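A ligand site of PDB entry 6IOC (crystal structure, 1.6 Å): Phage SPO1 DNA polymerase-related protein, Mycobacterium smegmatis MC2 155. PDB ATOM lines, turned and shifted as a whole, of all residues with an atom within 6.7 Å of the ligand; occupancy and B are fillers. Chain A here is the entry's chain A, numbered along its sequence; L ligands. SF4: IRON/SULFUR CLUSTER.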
ATOM      1  N   GLY A   6     -16.009  16.608  37.916  1.00  0.00           N
ATOM      2  CA  GLY A   6     -15.563  16.548  36.531  1.00  0.00           C
ATOM      3  C   GLY A   6     -16.744  16.342  35.598  1.00  0.00           C
ATOM      4  O   GLY A   6     -17.768  17.017  35.689  1.00  0.00           O
ATOM      5  N   ALA A   7     -16.593  15.401  34.672  1.00  0.00           N
ATOM      6  CA  ALA A   7     -17.563  15.207  33.602  1.00  0.00           C
ATOM      7  C   ALA A   7     -18.885  14.573  34.075  1.00  0.00           C
ATOM      8  O   ALA A   7     -19.855  14.563  33.312  1.00  0.00           O
ATOM      9  CB  ALA A   7     -16.923  14.326  32.503  1.00  0.00           C
ATOM     10  N   PHE A  10     -22.060  16.190  33.173  1.00  0.00           N
ATOM     11  CA  PHE A  10     -22.309  16.402  31.771  1.00  0.00           C
ATOM     12  C   PHE A  10     -22.721  15.130  31.027  1.00  0.00           C
ATOM     13  O   PHE A  10     -23.117  15.194  29.855  1.00  0.00           O
ATOM     14  CB  PHE A  10     -21.055  17.026  31.146  1.00  0.00           C
ATOM     15  CG  PHE A  10     -20.766  18.419  31.648  1.00  0.00           C
ATOM     16  CD1 PHE A  10     -21.433  19.501  31.086  1.00  0.00           C
ATOM     17  CD2 PHE A  10     -19.875  18.656  32.688  1.00  0.00           C
ATOM     18  CE1 PHE A  10     -21.213  20.807  31.550  1.00  0.00           C
ATOM     19  CE2 PHE A  10     -19.628  19.956  33.149  1.00  0.00           C
ATOM     20  CZ  PHE A  10     -20.313  21.028  32.574  1.00  0.00           C
ATOM     21  N   ALA A  24     -20.661  15.174  24.922  1.00  0.00           N
ATOM     22  CA  ALA A  24     -19.270  15.445  25.247  1.00  0.00           C
ATOM     23  C   ALA A  24     -18.798  16.746  24.634  1.00  0.00           C
ATOM     24  O   ALA A  24     -17.928  17.416  25.218  1.00  0.00           O
ATOM     25  CB  ALA A  24     -18.373  14.264  24.827  1.00  0.00           C
ATOM     26  N   GLY A  25     -19.407  17.174  23.512  1.00  0.00           N
ATOM     27  CA  GLY A  25     -19.024  18.489  23.000  1.00  0.00           C
ATOM     28  C   GLY A  25     -19.372  19.634  23.939  1.00  0.00           C
ATOM     29  O   GLY A  25     -18.722  20.685  23.870  1.00  0.00           O
ATOM     30  N   GLU A  26     -20.314  19.430  24.844  1.00  0.00           N
ATOM     31  CA  GLU A  26     -20.713  20.452  25.802  1.00  0.00           C
ATOM     32  C   GLU A  26     -19.973  20.337  27.109  1.00  0.00           C
ATOM     33  O   GLU A  26     -20.217  21.156  27.997  1.00  0.00           O
ATOM     34  CB  GLU A  26     -22.212  20.343  26.107  1.00  0.00           C
ATOM     35  CG  GLU A  26     -23.084  20.638  24.941  1.00  0.00           C
ATOM     36  CD  GLU A  26     -23.069  22.108  24.627  1.00  0.00           C
ATOM     37  OE1 GLU A  26     -23.806  22.852  25.280  1.00  0.00           O
ATOM     38  OE2 GLU A  26     -22.310  22.514  23.733  1.00  0.00           O
ATOM     39  N   CYS A  27     -19.152  19.310  27.287  1.00  0.00           N
ATOM     40  CA  CYS A  27     -18.537  19.079  28.588  1.00  0.00           C
ATOM     41  C   CYS A  27     -17.628  20.242  28.978  1.00  0.00           C
ATOM     42  O   CYS A  27     -16.842  20.731  28.152  1.00  0.00           O
ATOM     43  CB  CYS A  27     -17.745  17.776  28.542  1.00  0.00           C
ATOM     44  SG  CYS A  27     -17.169  17.258  30.125  1.00  0.00           S
ATOM     45  N   ARG A  28     -17.728  20.681  30.233  1.00  0.00           N
ATOM     46  CA  ARG A  28     -16.754  21.584  30.847  1.00  0.00           C
ATOM     47  C   ARG A  28     -16.187  20.963  32.121  1.00  0.00           C
ATOM     48  O   ARG A  28     -15.859  21.672  33.082  1.00  0.00           O
ATOM     49  CB  ARG A  28     -17.383  22.964  31.107  1.00  0.00           C
ATOM     50  CG  ARG A  28     -18.121  23.482  29.843  1.00  0.00           C
ATOM     51  CD  ARG A  28     -18.671  24.882  30.116  1.00  0.00           C
ATOM     52  NE  ARG A  28     -19.474  24.910  31.349  1.00  0.00           N
ATOM     53  CZ  ARG A  28     -20.785  24.715  31.377  1.00  0.00           C
ATOM     54  NH1 ARG A  28     -21.468  24.464  30.255  1.00  0.00           N
ATOM     55  NH2 ARG A  28     -21.425  24.753  32.535  1.00  0.00           N
ATOM     56  N   GLY A  29     -16.086  19.626  32.132  1.00  0.00           N
ATOM     57  CA  GLY A  29     -15.643  18.892  33.313  1.00  0.00           C
ATOM     58  C   GLY A  29     -14.241  19.223  33.761  1.00  0.00           C
ATOM     59  O   GLY A  29     -13.895  18.989  34.926  1.00  0.00           O
ATOM     60  N   CYS A  30     -13.387  19.715  32.868  1.00  0.00           N
ATOM     61  CA  CYS A  30     -12.057  20.173  33.221  1.00  0.00           C
ATOM     62  C   CYS A  30     -11.753  21.347  32.301  1.00  0.00           C
ATOM     63  O   CYS A  30     -12.618  21.793  31.541  1.00  0.00           O
ATOM     64  CB  CYS A  30     -11.044  19.032  33.162  1.00  0.00           C
ATOM     65  SG  CYS A  30     -10.477  18.517  31.531  1.00  0.00           S
ATOM     66  N   GLY A  31     -10.526  21.852  32.361  1.00  0.00           N
ATOM     67  CA  GLY A  31     -10.230  23.020  31.535  1.00  0.00           C
ATOM     68  C   GLY A  31      -9.984  22.740  30.069  1.00  0.00           C
ATOM     69  O   GLY A  31      -9.910  23.682  29.273  1.00  0.00           O
ATOM     70  N   LEU A  32      -9.846  21.469  29.668  1.00  0.00           N
ATOM     71  CA  LEU A  32      -9.294  21.192  28.355  1.00  0.00           C
ATOM     72  C   LEU A  32     -10.255  21.532  27.218  1.00  0.00           C
ATOM     73  O   LEU A  32      -9.817  21.625  26.059  1.00  0.00           O
ATOM     74  CB  LEU A  32      -8.856  19.713  28.277  1.00  0.00           C
ATOM     75  CG  LEU A  32      -7.724  19.333  29.228  1.00  0.00           C
ATOM     76  CD1 LEU A  32      -7.374  17.858  28.978  1.00  0.00           C
ATOM     77  CD2 LEU A  32      -6.509  20.201  28.964  1.00  0.00           C
ATOM     78  N   TYR A  33     -11.536  21.751  27.496  1.00  0.00           N
ATOM     79  CA  TYR A  33     -12.424  22.130  26.412  1.00  0.00           C
ATOM     80  C   TYR A  33     -12.077  23.501  25.830  1.00  0.00           C
ATOM     81  O   TYR A  33     -12.490  23.805  24.705  1.00  0.00           O
ATOM     82  CB  TYR A  33     -13.874  22.127  26.883  1.00  0.00           C
ATOM     83  CG  TYR A  33     -14.171  23.273  27.820  1.00  0.00           C
ATOM     84  CD1 TYR A  33     -14.702  24.458  27.343  1.00  0.00           C
ATOM     85  CD2 TYR A  33     -13.918  23.153  29.176  1.00  0.00           C
ATOM     86  CE1 TYR A  33     -14.954  25.520  28.203  1.00  0.00           C
ATOM     87  CE2 TYR A  33     -14.180  24.205  30.034  1.00  0.00           C
ATOM     88  CZ  TYR A  33     -14.691  25.394  29.533  1.00  0.00           C
ATOM     89  OH  TYR A  33     -14.959  26.456  30.370  1.00  0.00           O
ATOM     90  N   ARG A  34     -11.342  24.342  26.564  1.00  0.00           N
ATOM     91  CA  ARG A  34     -11.129  25.714  26.123  1.00  0.00           C
ATOM     92  C   ARG A  34     -10.169  25.796  24.933  1.00  0.00           C
ATOM     93  O   ARG A  34     -10.515  26.369  23.900  1.00  0.00           O
ATOM     94  CB  ARG A  34     -10.643  26.564  27.311  1.00  0.00           C
ATOM     95  CG  ARG A  34     -11.729  26.713  28.409  1.00  0.00           C
ATOM     96  CD  ARG A  34     -11.389  27.756  29.476  1.00  0.00           C
ATOM     97  NE  ARG A  34     -10.744  27.134  30.641  1.00  0.00           N
ATOM     98  CZ  ARG A  34     -11.296  27.008  31.840  1.00  0.00           C
ATOM     99  NH1 ARG A  34     -12.524  27.480  32.089  1.00  0.00           N
ATOM    100  NH2 ARG A  34     -10.622  26.426  32.817  1.00  0.00           N
ATOM    101  N   ALA A  39     -14.734  18.038  21.122  1.00  0.00           N
ATOM    102  CA  ALA A  39     -14.477  16.751  21.754  1.00  0.00           C
ATOM    103  C   ALA A  39     -14.241  15.709  20.670  1.00  0.00           C
ATOM    104  O   ALA A  39     -14.863  15.740  19.601  1.00  0.00           O
ATOM    105  CB  ALA A  39     -15.644  16.317  22.666  1.00  0.00           C
ATOM    106  N   ALA A  95      -8.525   8.327  26.787  1.00  0.00           N
ATOM    107  CA  ALA A  95      -8.808   8.623  28.193  1.00  0.00           C
ATOM    108  C   ALA A  95      -9.356  10.036  28.368  1.00  0.00           C
ATOM    109  O   ALA A  95     -10.239  10.277  29.187  1.00  0.00           O
ATOM    110  CB  ALA A  95      -7.533   8.448  29.031  1.00  0.00           C
ATOM    111  N   VAL A  96      -8.822  10.969  27.586  1.00  0.00           N
ATOM    112  CA  VAL A  96      -9.178  12.371  27.639  1.00  0.00           C
ATOM    113  C   VAL A  96      -9.733  12.752  26.276  1.00  0.00           C
ATOM    114  O   VAL A  96      -9.177  12.358  25.241  1.00  0.00           O
ATOM    115  CB  VAL A  96      -7.917  13.182  28.034  1.00  0.00           C
ATOM    116  CG1 VAL A  96      -8.037  14.633  27.740  1.00  0.00           C
ATOM    117  CG2 VAL A  96      -7.658  12.926  29.516  1.00  0.00           C
ATOM    118  N   LYS A  97     -10.845  13.493  26.249  1.00  0.00           N
ATOM    119  CA  LYS A  97     -11.583  13.735  25.020  1.00  0.00           C
ATOM    120  C   LYS A  97     -11.286  15.073  24.386  1.00  0.00           C
ATOM    121  O   LYS A  97     -11.700  15.290  23.245  1.00  0.00           O
ATOM    122  CB  LYS A  97     -13.095  13.628  25.256  1.00  0.00           C
ATOM    123  CG  LYS A  97     -13.653  12.285  25.852  1.00  0.00           C
ATOM    124  CD  LYS A  97     -13.234  11.059  25.107  1.00  0.00           C
ATOM    125  CE  LYS A  97     -14.212   9.873  25.310  1.00  0.00           C
ATOM    126  NZ  LYS A  97     -13.532   8.865  26.151  1.00  0.00           N
ATOM    127  N   HIS A  98     -10.570  15.971  25.073  1.00  0.00           N
ATOM    128  CA  HIS A  98     -10.164  17.235  24.474  1.00  0.00           C
ATOM    129  C   HIS A  98      -8.646  17.345  24.374  1.00  0.00           C
ATOM    130  O   HIS A  98      -7.937  17.080  25.352  1.00  0.00           O
ATOM    131  CB  HIS A  98     -10.733  18.438  25.233  1.00  0.00           C
ATOM    132  CG  HIS A  98     -12.196  18.668  24.996  1.00  0.00           C
ATOM    133  ND1 HIS A  98     -13.163  18.306  25.902  1.00  0.00           N
ATOM    134  CD2 HIS A  98     -12.859  19.209  23.940  1.00  0.00           C
ATOM    135  CE1 HIS A  98     -14.359  18.634  25.444  1.00  0.00           C
ATOM    136  NE2 HIS A  98     -14.196  19.189  24.250  1.00  0.00           N
ATOM    137  N   PHE A  99      -8.168  17.725  23.186  1.00  0.00           N
ATOM    138  CA  PHE A  99      -6.739  17.902  22.896  1.00  0.00           C
ATOM    139  C   PHE A  99      -6.104  18.910  23.844  1.00  0.00           C
ATOM    140  O   PHE A  99      -6.543  20.059  23.922  1.00  0.00           O
ATOM    141  CB  PHE A  99      -6.677  18.356  21.434  1.00  0.00           C
ATOM    142  CG  PHE A  99      -5.291  18.580  20.861  1.00  0.00           C
ATOM    143  CD1 PHE A  99      -4.198  17.789  21.209  1.00  0.00           C
ATOM    144  CD2 PHE A  99      -5.106  19.575  19.924  1.00  0.00           C
ATOM    145  CE1 PHE A  99      -2.946  18.006  20.629  1.00  0.00           C
ATOM    146  CE2 PHE A  99      -3.860  19.799  19.339  1.00  0.00           C
ATOM    147  CZ  PHE A  99      -2.793  19.011  19.706  1.00  0.00           C
ATOM    148  N   GLU A 119      -7.279  15.854  35.171  1.00  0.00           N
ATOM    149  CA  GLU A 119      -8.069  15.886  33.944  1.00  0.00           C
ATOM    150  C   GLU A 119      -8.496  14.484  33.552  1.00  0.00           C
ATOM    151  O   GLU A 119      -9.642  14.265  33.127  1.00  0.00           O
ATOM    152  CB  GLU A 119      -7.258  16.558  32.811  1.00  0.00           C
ATOM    153  CG  GLU A 119      -7.084  18.071  33.011  1.00  0.00           C
ATOM    154  CD  GLU A 119      -5.824  18.675  32.418  1.00  0.00           C
ATOM    155  OE1 GLU A 119      -4.889  17.967  32.006  1.00  0.00           O
ATOM    156  OE2 GLU A 119      -5.776  19.931  32.420  1.00  0.00           O
ATOM    157  N   VAL A 121      -9.023  11.929  35.559  1.00  0.00           N
ATOM    158  CA  VAL A 121     -10.127  11.498  36.433  1.00  0.00           C
ATOM    159  C   VAL A 121     -11.398  12.290  36.128  1.00  0.00           C
ATOM    160  O   VAL A 121     -12.513  11.755  36.187  1.00  0.00           O
ATOM    161  CB  VAL A 121      -9.703  11.641  37.910  1.00  0.00           C
ATOM    162  CG1 VAL A 121     -10.856  11.297  38.803  1.00  0.00           C
ATOM    163  CG2 VAL A 121      -8.535  10.703  38.202  1.00  0.00           C
ATOM    164  N   ALA A 122     -11.257  13.552  35.757  1.00  0.00           N
ATOM    165  CA  ALA A 122     -12.425  14.340  35.394  1.00  0.00           C
ATOM    166  C   ALA A 122     -13.139  13.762  34.180  1.00  0.00           C
ATOM    167  O   ALA A 122     -14.378  13.804  34.104  1.00  0.00           O
ATOM    168  CB  ALA A 122     -11.996  15.781  35.128  1.00  0.00           C
ATOM    169  N   CYS A 123     -12.376  13.197  33.237  1.00  0.00           N
ATOM    170  CA  CYS A 123     -12.932  12.742  31.970  1.00  0.00           C
ATOM    171  C   CYS A 123     -13.363  11.274  32.037  1.00  0.00           C
ATOM    172  O   CYS A 123     -14.189  10.836  31.220  1.00  0.00           O
ATOM    173  CB  CYS A 123     -11.906  12.976  30.855  1.00  0.00           C
ATOM    174  SG  CYS A 123     -12.620  13.104  29.231  1.00  0.00           S
ATOM    175  N   ARG A 124     -12.868  10.529  33.013  1.00  0.00           N
ATOM    176  CA  ARG A 124     -13.184   9.114  33.162  1.00  0.00           C
ATOM    177  C   ARG A 124     -14.680   8.764  33.114  1.00  0.00           C
ATOM    178  O   ARG A 124     -15.015   7.695  32.577  1.00  0.00           O
ATOM    179  CB  ARG A 124     -12.557   8.609  34.462  1.00  0.00           C
ATOM    180  CG  ARG A 124     -12.630   7.100  34.635  1.00  0.00           C
ATOM    181  CD  ARG A 124     -11.891   6.695  35.933  1.00  0.00           C
ATOM    182  NE  ARG A 124     -11.971   5.262  36.233  1.00  0.00           N
ATOM    183  CZ  ARG A 124     -13.014   4.704  36.827  1.00  0.00           C
ATOM    184  NH1 ARG A 124     -13.015   3.401  37.078  1.00  0.00           N
ATOM    185  NH2 ARG A 124     -14.093   5.432  37.125  1.00  0.00           N
ATOM    186  N   PRO A 125     -15.615   9.619  33.614  1.00  0.00           N
ATOM    187  CA  PRO A 125     -17.039   9.278  33.435  1.00  0.00           C
ATOM    188  C   PRO A 125     -17.451   8.998  31.985  1.00  0.00           C
ATOM    189  O   PRO A 125     -18.384   8.205  31.762  1.00  0.00           O
ATOM    190  CB  PRO A 125     -17.765  10.505  34.011  1.00  0.00           C
ATOM    191  CG  PRO A 125     -16.797  11.012  35.083  1.00  0.00           C
ATOM    192  CD  PRO A 125     -15.465  10.839  34.435  1.00  0.00           C
ATOM    193  N   TRP A 126     -16.781   9.637  30.999  1.00  0.00           N
ATOM    194  CA  TRP A 126     -17.102   9.321  29.596  1.00  0.00           C
ATOM    195  C   TRP A 126     -16.663   7.912  29.255  1.00  0.00           C
ATOM    196  O   TRP A 126     -17.393   7.201  28.552  1.00  0.00           O
ATOM    197  CB  TRP A 126     -16.448  10.303  28.630  1.00  0.00           C
ATOM    198  CG  TRP A 126     -17.021  11.689  28.754  1.00  0.00           C
ATOM    199  CD1 TRP A 126     -16.367  12.804  29.216  1.00  0.00           C
ATOM    200  CD2 TRP A 126     -18.364  12.115  28.422  1.00  0.00           C
ATOM    201  NE1 TRP A 126     -17.223  13.901  29.194  1.00  0.00           N
ATOM    202  CE2 TRP A 126     -18.453  13.499  28.743  1.00  0.00           C
ATOM    203  CE3 TRP A 126     -19.492  11.469  27.912  1.00  0.00           C
ATOM    204  CZ2 TRP A 126     -19.597  14.240  28.528  1.00  0.00           C
ATOM    205  CZ3 TRP A 126     -20.636  12.211  27.698  1.00  0.00           C
ATOM    206  CH2 TRP A 126     -20.694  13.591  28.041  1.00  0.00           C
HETATM  207 FE1  SF4 L   1     -13.032  15.303  29.231  1.00  0.00          FE
HETATM  208 FE2  SF4 L   1     -14.861  17.178  29.737  1.00  0.00          FE
HETATM  209 FE3  SF4 L   1     -13.119  17.585  27.819  1.00  0.00          FE
HETATM  210 FE4  SF4 L   1     -12.293  17.667  30.351  1.00  0.00          FE
HETATM  211  S1  SF4 L   1     -13.726  19.056  29.368  1.00  0.00           S
HETATM  212  S2  SF4 L   1     -11.323  16.564  28.565  1.00  0.00           S
HETATM  213  S3  SF4 L   1     -13.607  16.177  31.244  1.00  0.00           S
HETATM  214  S4  SF4 L   1     -14.610  15.951  27.862  1.00  0.00           S
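The backbone NH of His 98 lies close to a sulfur (S2) of the ligand (3.6 Å).
An iron atom (FE3) of the ligand is bound by a ring nitrogen (ND1) of His 98.
The backbone NH of Cys 123 lies close to a sulfur (S3) of the ligand.
The side-chain sulfur of Cys 123 is bound to an iron atom (FE1) of the ligand, 2.2 Å away.
N of Cys 30 sits close to S1 of the ligand, 3.6 Å away.
SG of Cys 30 binds FE4 of the ligand (2.3 Å).
FE2 of the ligand is bound by SG of Cys 27 (2.3 Å).
The indole nitrogen of Trp 126 sits close to a sulfur (S4) of the ligand.
S1 of the ligand sits close to N of Gly 29, 3.7 Å away.
N of Ala 39 sits at hydrogen-bond distance from NE2 of His 98 (3.4 Å).
The backbone NH of Lys 97 lies close to the side-chain sulfur of Cys 123 (3.5 Å).
The side-chain sulfur (SG) of Cys 123 sits close to the backbone carbonyl oxygen (O) of Ala 95 (3.7 Å).
The side-chain sulfur of Cys 30 sits close to the backbone NH of Leu 32 (3.5 Å).
The side-chain sulfur of Cys 27 sits close to the indole nitrogen of Trp 126 (3.5 Å).
SG of Cys 27 lies close to N of Gly 29.
The backbone carbonyl oxygen (O) of Ala 122 is in hydrogen-bond range of the backbone NH (N) of Ala 7 (2.8 Å).
The guanidinium group (NH1) of Arg 34 lies within hydrogen-bond range of the side-chain hydroxyl (OH) of Tyr 33, at 3.2 Å.
The backbone carbonyl oxygen (O) of Ala 122 sits close to a sulfur (S3) of the ligand, at 3.8 Å.
Tyr 33 touches the ligand (N to S1, 3.9 Å).
Val 96 touches the ligand.
CB of Lys 97 touches S4 of the ligand (3.8 Å).
Ten residues have an atom within 4 Å of the ligand: Cys 27, Gly 29, Cys 30, Tyr 33, Val 96, Lys 97, His 98, Ala 122, Cys 123 and Trp 126.
The nearest printed residue that does not touch the ligand is Ala 7 (4.001 Å).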
